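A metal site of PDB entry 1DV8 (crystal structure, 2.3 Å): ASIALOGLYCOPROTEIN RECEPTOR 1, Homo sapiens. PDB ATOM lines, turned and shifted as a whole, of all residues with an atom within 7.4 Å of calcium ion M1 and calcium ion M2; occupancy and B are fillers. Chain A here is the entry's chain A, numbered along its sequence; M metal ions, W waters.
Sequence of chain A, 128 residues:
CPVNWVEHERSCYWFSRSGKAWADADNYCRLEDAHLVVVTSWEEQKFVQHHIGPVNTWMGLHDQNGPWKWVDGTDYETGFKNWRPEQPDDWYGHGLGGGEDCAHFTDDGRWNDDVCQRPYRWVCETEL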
ATOM      1  N   HIS A  62     -21.377 -20.584  21.548  1.00  0.00           N
ATOM      2  CA  HIS A  62     -21.668 -20.908  20.157  1.00  0.00           C
ATOM      3  C   HIS A  62     -20.911 -22.144  19.729  1.00  0.00           C
ATOM      4  O   HIS A  62     -19.931 -22.540  20.392  1.00  0.00           O
ATOM      5  CB  HIS A  62     -21.267 -19.734  19.244  1.00  0.00           C
ATOM      6  CG  HIS A  62     -19.780 -19.548  19.148  1.00  0.00           C
ATOM      7  ND1 HIS A  62     -19.009 -20.191  18.199  1.00  0.00           N
ATOM      8  CD2 HIS A  62     -18.917 -18.857  19.924  1.00  0.00           C
ATOM      9  CE1 HIS A  62     -17.736 -19.920  18.409  1.00  0.00           C
ATOM     10  NE2 HIS A  62     -17.649 -19.110  19.457  1.00  0.00           N
ATOM     11  N   ASP A  63     -21.347 -22.758  18.636  1.00  0.00           N
ATOM     12  CA  ASP A  63     -20.681 -23.928  18.100  1.00  0.00           C
ATOM     13  C   ASP A  63     -20.389 -23.685  16.620  1.00  0.00           C
ATOM     14  O   ASP A  63     -20.378 -24.602  15.813  1.00  0.00           O
ATOM     15  CB  ASP A  63     -21.539 -25.192  18.310  1.00  0.00           C
ATOM     16  CG  ASP A  63     -22.736 -25.274  17.376  1.00  0.00           C
ATOM     17  OD1 ASP A  63     -23.155 -24.221  16.849  1.00  0.00           O
ATOM     18  OD2 ASP A  63     -23.247 -26.404  17.205  1.00  0.00           O
ATOM     19  N   GLN A  64     -20.144 -22.418  16.300  1.00  0.00           N
ATOM     20  CA  GLN A  64     -19.851 -21.986  14.940  1.00  0.00           C
ATOM     21  C   GLN A  64     -18.581 -22.589  14.364  1.00  0.00           C
ATOM     22  O   GLN A  64     -18.458 -22.717  13.139  1.00  0.00           O
ATOM     23  CB  GLN A  64     -19.718 -20.462  14.896  1.00  0.00           C
ATOM     24  CG  GLN A  64     -21.026 -19.690  14.935  1.00  0.00           C
ATOM     25  CD  GLN A  64     -20.826 -18.260  15.417  1.00  0.00           C
ATOM     26  OE1 GLN A  64     -20.661 -17.988  16.619  1.00  0.00           O
ATOM     27  NE2 GLN A  64     -20.823 -17.342  14.473  1.00  0.00           N
ATOM     28  N   GLY A  66     -17.412 -25.568  15.504  1.00  0.00           N
ATOM     29  CA  GLY A  66     -17.403 -26.978  15.821  1.00  0.00           C
ATOM     30  C   GLY A  66     -17.954 -27.240  17.209  1.00  0.00           C
ATOM     31  O   GLY A  66     -19.160 -27.265  17.397  1.00  0.00           O
ATOM     32  N   TRP A  68     -18.911 -26.704  21.301  1.00  0.00           N
ATOM     33  CA  TRP A  68     -19.396 -25.600  22.097  1.00  0.00           C
ATOM     34  C   TRP A  68     -18.224 -24.941  22.797  1.00  0.00           C
ATOM     35  O   TRP A  68     -17.373 -25.618  23.381  1.00  0.00           O
ATOM     36  CB  TRP A  68     -20.436 -26.086  23.107  1.00  0.00           C
ATOM     37  CG  TRP A  68     -21.767 -26.355  22.477  1.00  0.00           C
ATOM     38  CD1 TRP A  68     -22.325 -27.575  22.229  1.00  0.00           C
ATOM     39  CD2 TRP A  68     -22.669 -25.381  21.934  1.00  0.00           C
ATOM     40  NE1 TRP A  68     -23.530 -27.421  21.563  1.00  0.00           N
ATOM     41  CE2 TRP A  68     -23.761 -26.084  21.370  1.00  0.00           C
ATOM     42  CE3 TRP A  68     -22.653 -23.980  21.863  1.00  0.00           C
ATOM     43  CZ2 TRP A  68     -24.829 -25.439  20.742  1.00  0.00           C
ATOM     44  CZ3 TRP A  68     -23.720 -23.332  21.245  1.00  0.00           C
ATOM     45  CH2 TRP A  68     -24.796 -24.060  20.686  1.00  0.00           C
ATOM     46  N   TRP A  83     -29.497 -26.001  29.605  1.00  0.00           N
ATOM     47  CA  TRP A  83     -30.257 -26.127  28.371  1.00  0.00           C
ATOM     48  C   TRP A  83     -31.724 -26.454  28.597  1.00  0.00           C
ATOM     49  O   TRP A  83     -32.118 -27.080  29.571  1.00  0.00           O
ATOM     50  CB  TRP A  83     -29.667 -27.210  27.422  1.00  0.00           C
ATOM     51  CG  TRP A  83     -28.297 -26.948  26.916  1.00  0.00           C
ATOM     52  CD1 TRP A  83     -27.134 -27.485  27.387  1.00  0.00           C
ATOM     53  CD2 TRP A  83     -27.921 -26.069  25.839  1.00  0.00           C
ATOM     54  NE1 TRP A  83     -26.070 -27.008  26.677  1.00  0.00           N
ATOM     55  CE2 TRP A  83     -26.525 -26.142  25.724  1.00  0.00           C
ATOM     56  CE3 TRP A  83     -28.647 -25.243  24.966  1.00  0.00           C
ATOM     57  CZ2 TRP A  83     -25.825 -25.410  24.779  1.00  0.00           C
ATOM     58  CZ3 TRP A  83     -27.942 -24.519  24.022  1.00  0.00           C
ATOM     59  CH2 TRP A  83     -26.548 -24.611  23.936  1.00  0.00           C
ATOM     60  N   GLU A  86     -34.564 -30.917  25.236  1.00  0.00           N
ATOM     61  CA  GLU A  86     -34.483 -31.158  23.801  1.00  0.00           C
ATOM     62  C   GLU A  86     -33.607 -30.140  23.051  1.00  0.00           C
ATOM     63  O   GLU A  86     -33.713 -30.002  21.836  1.00  0.00           O
ATOM     64  CB  GLU A  86     -35.880 -31.166  23.195  1.00  0.00           C
ATOM     65  CG  GLU A  86     -36.854 -32.066  23.940  1.00  0.00           C
ATOM     66  CD  GLU A  86     -38.270 -31.953  23.406  1.00  0.00           C
ATOM     67  OE1 GLU A  86     -38.542 -32.526  22.323  1.00  0.00           O
ATOM     68  OE2 GLU A  86     -39.107 -31.297  24.073  1.00  0.00           O
ATOM     69  N   GLN A  87     -32.756 -29.420  23.777  1.00  0.00           N
ATOM     70  CA  GLN A  87     -31.843 -28.461  23.157  1.00  0.00           C
ATOM     71  C   GLN A  87     -30.437 -28.731  23.704  1.00  0.00           C
ATOM     72  O   GLN A  87     -30.296 -29.237  24.808  1.00  0.00           O
ATOM     73  CB  GLN A  87     -32.277 -27.029  23.481  1.00  0.00           C
ATOM     74  CG  GLN A  87     -33.677 -26.666  23.032  1.00  0.00           C
ATOM     75  CD  GLN A  87     -33.880 -26.726  21.518  1.00  0.00           C
ATOM     76  OE1 GLN A  87     -32.935 -26.715  20.726  1.00  0.00           O
ATOM     77  NE2 GLN A  87     -35.133 -26.773  21.117  1.00  0.00           N
ATOM     78  N   PRO A  88     -29.391 -28.408  22.932  1.00  0.00           N
ATOM     79  CA  PRO A  88     -29.403 -27.812  21.592  1.00  0.00           C
ATOM     80  C   PRO A  88     -29.909 -28.830  20.578  1.00  0.00           C
ATOM     81  O   PRO A  88     -29.665 -30.036  20.734  1.00  0.00           O
ATOM     82  CB  PRO A  88     -27.923 -27.483  21.340  1.00  0.00           C
ATOM     83  CG  PRO A  88     -27.258 -27.592  22.688  1.00  0.00           C
ATOM     84  CD  PRO A  88     -28.021 -28.681  23.391  1.00  0.00           C
ATOM     85  N   ASP A  89     -30.569 -28.355  19.516  1.00  0.00           N
ATOM     86  CA  ASP A  89     -31.078 -29.268  18.510  1.00  0.00           C
ATOM     87  C   ASP A  89     -30.633 -28.937  17.071  1.00  0.00           C
ATOM     88  O   ASP A  89     -31.049 -29.603  16.132  1.00  0.00           O
ATOM     89  CB  ASP A  89     -32.600 -29.315  18.579  1.00  0.00           C
ATOM     90  CG  ASP A  89     -33.237 -28.049  18.054  1.00  0.00           C
ATOM     91  OD1 ASP A  89     -32.465 -27.091  17.807  1.00  0.00           O
ATOM     92  OD2 ASP A  89     -34.483 -27.997  17.901  1.00  0.00           O
ATOM     93  N   ASP A  90     -29.806 -27.916  16.918  1.00  0.00           N
ATOM     94  CA  ASP A  90     -29.280 -27.525  15.601  1.00  0.00           C
ATOM     95  C   ASP A  90     -30.297 -27.586  14.463  1.00  0.00           C
ATOM     96  O   ASP A  90     -29.985 -28.049  13.361  1.00  0.00           O
ATOM     97  CB  ASP A  90     -28.051 -28.383  15.242  1.00  0.00           C
ATOM     98  CG  ASP A  90     -27.126 -27.723  14.201  1.00  0.00           C
ATOM     99  OD1 ASP A  90     -26.745 -26.553  14.368  1.00  0.00           O
ATOM    100  OD2 ASP A  90     -26.762 -28.382  13.207  1.00  0.00           O
ATOM    101  N   TRP A  91     -31.501 -27.094  14.746  1.00  0.00           N
ATOM    102  CA  TRP A  91     -32.609 -27.068  13.786  1.00  0.00           C
ATOM    103  C   TRP A  91     -32.323 -26.339  12.456  1.00  0.00           C
ATOM    104  O   TRP A  91     -31.695 -25.287  12.408  1.00  0.00           O
ATOM    105  CB  TRP A  91     -33.822 -26.416  14.439  1.00  0.00           C
ATOM    106  CG  TRP A  91     -35.079 -26.564  13.651  1.00  0.00           C
ATOM    107  CD1 TRP A  91     -35.554 -27.704  13.073  1.00  0.00           C
ATOM    108  CD2 TRP A  91     -36.086 -25.552  13.447  1.00  0.00           C
ATOM    109  NE1 TRP A  91     -36.801 -27.479  12.535  1.00  0.00           N
ATOM    110  CE2 TRP A  91     -37.146 -26.169  12.748  1.00  0.00           C
ATOM    111  CE3 TRP A  91     -36.191 -24.202  13.793  1.00  0.00           C
ATOM    112  CZ2 TRP A  91     -38.316 -25.462  12.384  1.00  0.00           C
ATOM    113  CZ3 TRP A  91     -37.360 -23.495  13.429  1.00  0.00           C
ATOM    114  CH2 TRP A  91     -38.406 -24.137  12.736  1.00  0.00           C
ATOM    115  N   TYR A  92     -32.812 -26.936  11.370  1.00  0.00           N
ATOM    116  CA  TYR A  92     -32.667 -26.387  10.029  1.00  0.00           C
ATOM    117  C   TYR A  92     -34.037 -25.954   9.482  1.00  0.00           C
ATOM    118  O   TYR A  92     -34.101 -25.158   8.543  1.00  0.00           O
ATOM    119  CB  TYR A  92     -32.071 -27.445   9.070  1.00  0.00           C
ATOM    120  CG  TYR A  92     -30.561 -27.575   9.097  1.00  0.00           C
ATOM    121  CD1 TYR A  92     -29.896 -28.084  10.214  1.00  0.00           C
ATOM    122  CD2 TYR A  92     -29.788 -27.145   8.010  1.00  0.00           C
ATOM    123  CE1 TYR A  92     -28.495 -28.184  10.247  1.00  0.00           C
ATOM    124  CE2 TYR A  92     -28.386 -27.236   8.029  1.00  0.00           C
ATOM    125  CZ  TYR A  92     -27.752 -27.749   9.154  1.00  0.00           C
ATOM    126  OH  TYR A  92     -26.377 -27.839   9.137  1.00  0.00           O
ATOM    127  N   GLY A  99     -27.888 -24.586  10.300  1.00  0.00           N
ATOM    128  CA  GLY A  99     -28.545 -25.116  11.480  1.00  0.00           C
ATOM    129  C   GLY A  99     -28.738 -23.979  12.464  1.00  0.00           C
ATOM    130  O   GLY A  99     -29.300 -22.971  12.085  1.00  0.00           O
ATOM    131  N   GLU A 100     -28.265 -24.152  13.708  1.00  0.00           N
ATOM    132  CA  GLU A 100     -28.350 -23.136  14.772  1.00  0.00           C
ATOM    133  C   GLU A 100     -27.047 -23.213  15.593  1.00  0.00           C
ATOM    134  O   GLU A 100     -26.762 -24.227  16.249  1.00  0.00           O
ATOM    135  CB  GLU A 100     -29.574 -23.414  15.659  1.00  0.00           C
ATOM    136  CG  GLU A 100     -30.912 -23.167  14.962  1.00  0.00           C
ATOM    137  CD  GLU A 100     -32.113 -23.608  15.791  1.00  0.00           C
ATOM    138  OE1 GLU A 100     -33.215 -23.046  15.634  1.00  0.00           O
ATOM    139  OE2 GLU A 100     -31.973 -24.536  16.605  1.00  0.00           O
ATOM    140  N   ASP A 101     -26.259 -22.149  15.544  1.00  0.00           N
ATOM    141  CA  ASP A 101     -24.969 -22.124  16.203  1.00  0.00           C
ATOM    142  C   ASP A 101     -24.776 -21.137  17.348  1.00  0.00           C
ATOM    143  O   ASP A 101     -23.689 -21.034  17.879  1.00  0.00           O
ATOM    144  CB  ASP A 101     -23.880 -21.873  15.163  1.00  0.00           C
ATOM    145  CG  ASP A 101     -23.968 -22.833  14.015  1.00  0.00           C
ATOM    146  OD1 ASP A 101     -24.515 -23.929  14.254  1.00  0.00           O
ATOM    147  OD2 ASP A 101     -23.483 -22.498  12.901  1.00  0.00           O
ATOM    148  N   CYS A 102     -25.809 -20.398  17.711  1.00  0.00           N
ATOM    149  CA  CYS A 102     -25.619 -19.437  18.790  1.00  0.00           C
ATOM    150  C   CYS A 102     -26.605 -19.706  19.908  1.00  0.00           C
ATOM    151  O   CYS A 102     -27.795 -19.958  19.660  1.00  0.00           O
ATOM    152  CB  CYS A 102     -25.757 -18.021  18.232  1.00  0.00           C
ATOM    153  SG  CYS A 102     -24.308 -17.548  17.233  1.00  0.00           S
ATOM    154  N   HIS A 104     -28.803 -18.741  23.271  1.00  0.00           N
ATOM    155  CA  HIS A 104     -29.488 -17.608  23.858  1.00  0.00           C
ATOM    156  C   HIS A 104     -30.422 -18.085  24.958  1.00  0.00           C
ATOM    157  O   HIS A 104     -30.933 -19.210  24.937  1.00  0.00           O
ATOM    158  CB  HIS A 104     -30.282 -16.863  22.780  1.00  0.00           C
ATOM    159  CG  HIS A 104     -31.549 -17.548  22.362  1.00  0.00           C
ATOM    160  ND1 HIS A 104     -32.759 -17.324  22.988  1.00  0.00           N
ATOM    161  CD2 HIS A 104     -31.801 -18.424  21.356  1.00  0.00           C
ATOM    162  CE1 HIS A 104     -33.705 -18.021  22.375  1.00  0.00           C
ATOM    163  NE2 HIS A 104     -33.147 -18.705  21.385  1.00  0.00           N
ATOM    164  N   TRP A 111     -31.535 -22.219  28.102  1.00  0.00           N
ATOM    165  CA  TRP A 111     -30.897 -21.966  26.825  1.00  0.00           C
ATOM    166  C   TRP A 111     -31.456 -22.710  25.623  1.00  0.00           C
ATOM    167  O   TRP A 111     -32.045 -23.770  25.751  1.00  0.00           O
ATOM    168  CB  TRP A 111     -29.398 -22.249  26.952  1.00  0.00           C
ATOM    169  CG  TRP A 111     -28.763 -21.776  28.228  1.00  0.00           C
ATOM    170  CD1 TRP A 111     -29.230 -20.829  29.074  1.00  0.00           C
ATOM    171  CD2 TRP A 111     -27.471 -22.180  28.740  1.00  0.00           C
ATOM    172  NE1 TRP A 111     -28.323 -20.610  30.087  1.00  0.00           N
ATOM    173  CE2 TRP A 111     -27.236 -21.425  29.900  1.00  0.00           C
ATOM    174  CE3 TRP A 111     -26.509 -23.101  28.328  1.00  0.00           C
ATOM    175  CZ2 TRP A 111     -26.065 -21.559  30.654  1.00  0.00           C
ATOM    176  CZ3 TRP A 111     -25.340 -23.238  29.072  1.00  0.00           C
ATOM    177  CH2 TRP A 111     -25.141 -22.473  30.216  1.00  0.00           C
ATOM    178  N   ASN A 112     -31.255 -22.130  24.452  1.00  0.00           N
ATOM    179  CA  ASN A 112     -31.673 -22.731  23.187  1.00  0.00           C
ATOM    180  C   ASN A 112     -30.669 -22.264  22.127  1.00  0.00           C
ATOM    181  O   ASN A 112     -30.146 -21.155  22.215  1.00  0.00           O
ATOM    182  CB  ASN A 112     -33.080 -22.267  22.792  1.00  0.00           C
ATOM    183  CG  ASN A 112     -33.446 -22.678  21.373  1.00  0.00           C
ATOM    184  OD1 ASN A 112     -33.200 -23.806  20.948  1.00  0.00           O
ATOM    185  ND2 ASN A 112     -34.040 -21.757  20.641  1.00  0.00           N
ATOM    186  N   ASP A 113     -30.370 -23.113  21.149  1.00  0.00           N
ATOM    187  CA  ASP A 113     -29.452 -22.709  20.088  1.00  0.00           C
ATOM    188  C   ASP A 113     -30.369 -22.236  18.960  1.00  0.00           C
ATOM    189  O   ASP A 113     -31.396 -22.852  18.709  1.00  0.00           O
ATOM    190  CB  ASP A 113     -28.573 -23.885  19.653  1.00  0.00           C
ATOM    191  CG  ASP A 113     -29.375 -25.070  19.128  1.00  0.00           C
ATOM    192  OD1 ASP A 113     -30.584 -25.155  19.435  1.00  0.00           O
ATOM    193  OD2 ASP A 113     -28.764 -25.936  18.437  1.00  0.00           O
ATOM    194  N   ASP A 114     -29.990 -21.132  18.304  1.00  0.00           N
ATOM    195  CA  ASP A 114     -30.803 -20.547  17.242  1.00  0.00           C
ATOM    196  C   ASP A 114     -29.898 -19.932  16.156  1.00  0.00           C
ATOM    197  O   ASP A 114     -28.676 -19.853  16.325  1.00  0.00           O
ATOM    198  CB  ASP A 114     -31.707 -19.458  17.855  1.00  0.00           C
ATOM    199  CG  ASP A 114     -32.953 -19.202  17.045  1.00  0.00           C
ATOM    200  OD1 ASP A 114     -33.943 -18.681  17.612  1.00  0.00           O
ATOM    201  OD2 ASP A 114     -32.955 -19.521  15.830  1.00  0.00           O
ATOM    202  N   VAL A 115     -30.509 -19.480  15.068  1.00  0.00           N
ATOM    203  CA  VAL A 115     -29.821 -18.888  13.924  1.00  0.00           C
ATOM    204  C   VAL A 115     -29.074 -17.639  14.343  1.00  0.00           C
ATOM    205  O   VAL A 115     -29.681 -16.633  14.704  1.00  0.00           O
ATOM    206  CB  VAL A 115     -30.830 -18.549  12.810  1.00  0.00           C
ATOM    207  CG1 VAL A 115     -30.139 -17.849  11.662  1.00  0.00           C
ATOM    208  CG2 VAL A 115     -31.506 -19.826  12.329  1.00  0.00           C
HETATM  209 CA    CA M   1     -32.761 -24.854  18.809  1.00  0.00          CA
HETATM  210 CA    CA M   2     -24.920 -25.829  15.579  1.00  0.00          CA
HETATM  211  O   HOH W   1     -26.257 -26.566  17.313  1.00  0.00           O
HETATM  212  O   HOH W   2     -35.384 -25.575  18.187  1.00  0.00           O
HETATM  213  O   HOH W   3     -35.032 -23.262  17.635  1.00  0.00           O
HETATM  214  O   HOH W   4     -24.738 -28.054  15.795  1.00  0.00           O
HETATM  215  O   HOH W   5     -23.551 -26.608  13.975  1.00  0.00           O
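The side-chain carboxylate (OD2) of Asp 113 lies within hydrogen-bond range of the backbone NH (N) of Asp 90 (2.7 Å).
The backbone NH (N) of Asp 101 is in hydrogen-bond range of the backbone carbonyl oxygen (O) of Asp 114.
The side-chain carboxylate (OE2) of Glu 100 lies close to the backbone NH (N) of Trp 91 (3.2 Å).
N of His 104 is in hydrogen-bond range of O of Asn 112 (3.0 Å).
The backbone NH (N) of Trp 91 lies close to the side-chain carboxylate (OD1) of Asp 89.
Five residues have an atom within 4 Å of calcium ion M1: Gln 87, Asp 89, Glu 100, Asn 112 and Asp 113.
The nearest printed residue that does not touch calcium ion M1 is Asp 90 (4.7 Å).
Four residues have an atom within 4 Å of calcium ion M2: Asp 63, Asp 90, Glu 100 and Asp 101.
The nearest printed residue that does not touch calcium ion M2 is Asp 113 (4.8 Å).
Calcium ion M1 is bound by OD1 of Asp 113, at 2.3 Å.
The side-chain carboxylate (OE2) of Glu 100 binds calcium ion M1, 2.4 Å away.
OD1 of Asn 112 is bound to calcium ion M1, 2.4 Å away.
O of Asp 113 is bound to calcium ion M1 (2.4 Å).
OD1 of Asp 89 binds calcium ion M1, 2.5 Å away.
The side-chain amide oxygen (OE1) of Gln 87 binds calcium ion M1 (2.7 Å).
Water W2 is bound to calcium ion M1.
Calcium ion M1 has seven donor atoms within binding distance.
Slightly farther from calcium ion M1 lies water W3 (3.0 Å).
Water W4 is bound to calcium ion M2, at 2.2 Å.
Water W5 binds calcium ion M2 (2.2 Å).
OD1 of Asp 90 is bound to calcium ion M2.
Calcium ion M2 is bound by water W1, at 2.3 Å.
OD1 of Asp 101 binds calcium ion M2 (2.4 Å).
OD2 of Asp 63 binds calcium ion M2 (2.4 Å).
Calcium ion M2 is bound by O of Glu 100 (2.5 Å).
Calcium ion M2 is bound by OD1 of Asp 63 (2.7 Å).
Calcium ion M2 has eight donor atoms within binding distance.
Water W2 lies within hydrogen-bond range of OD2 of Asp 89 (2.6 Å) and NE2 of Gln 87 (3.2 Å).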
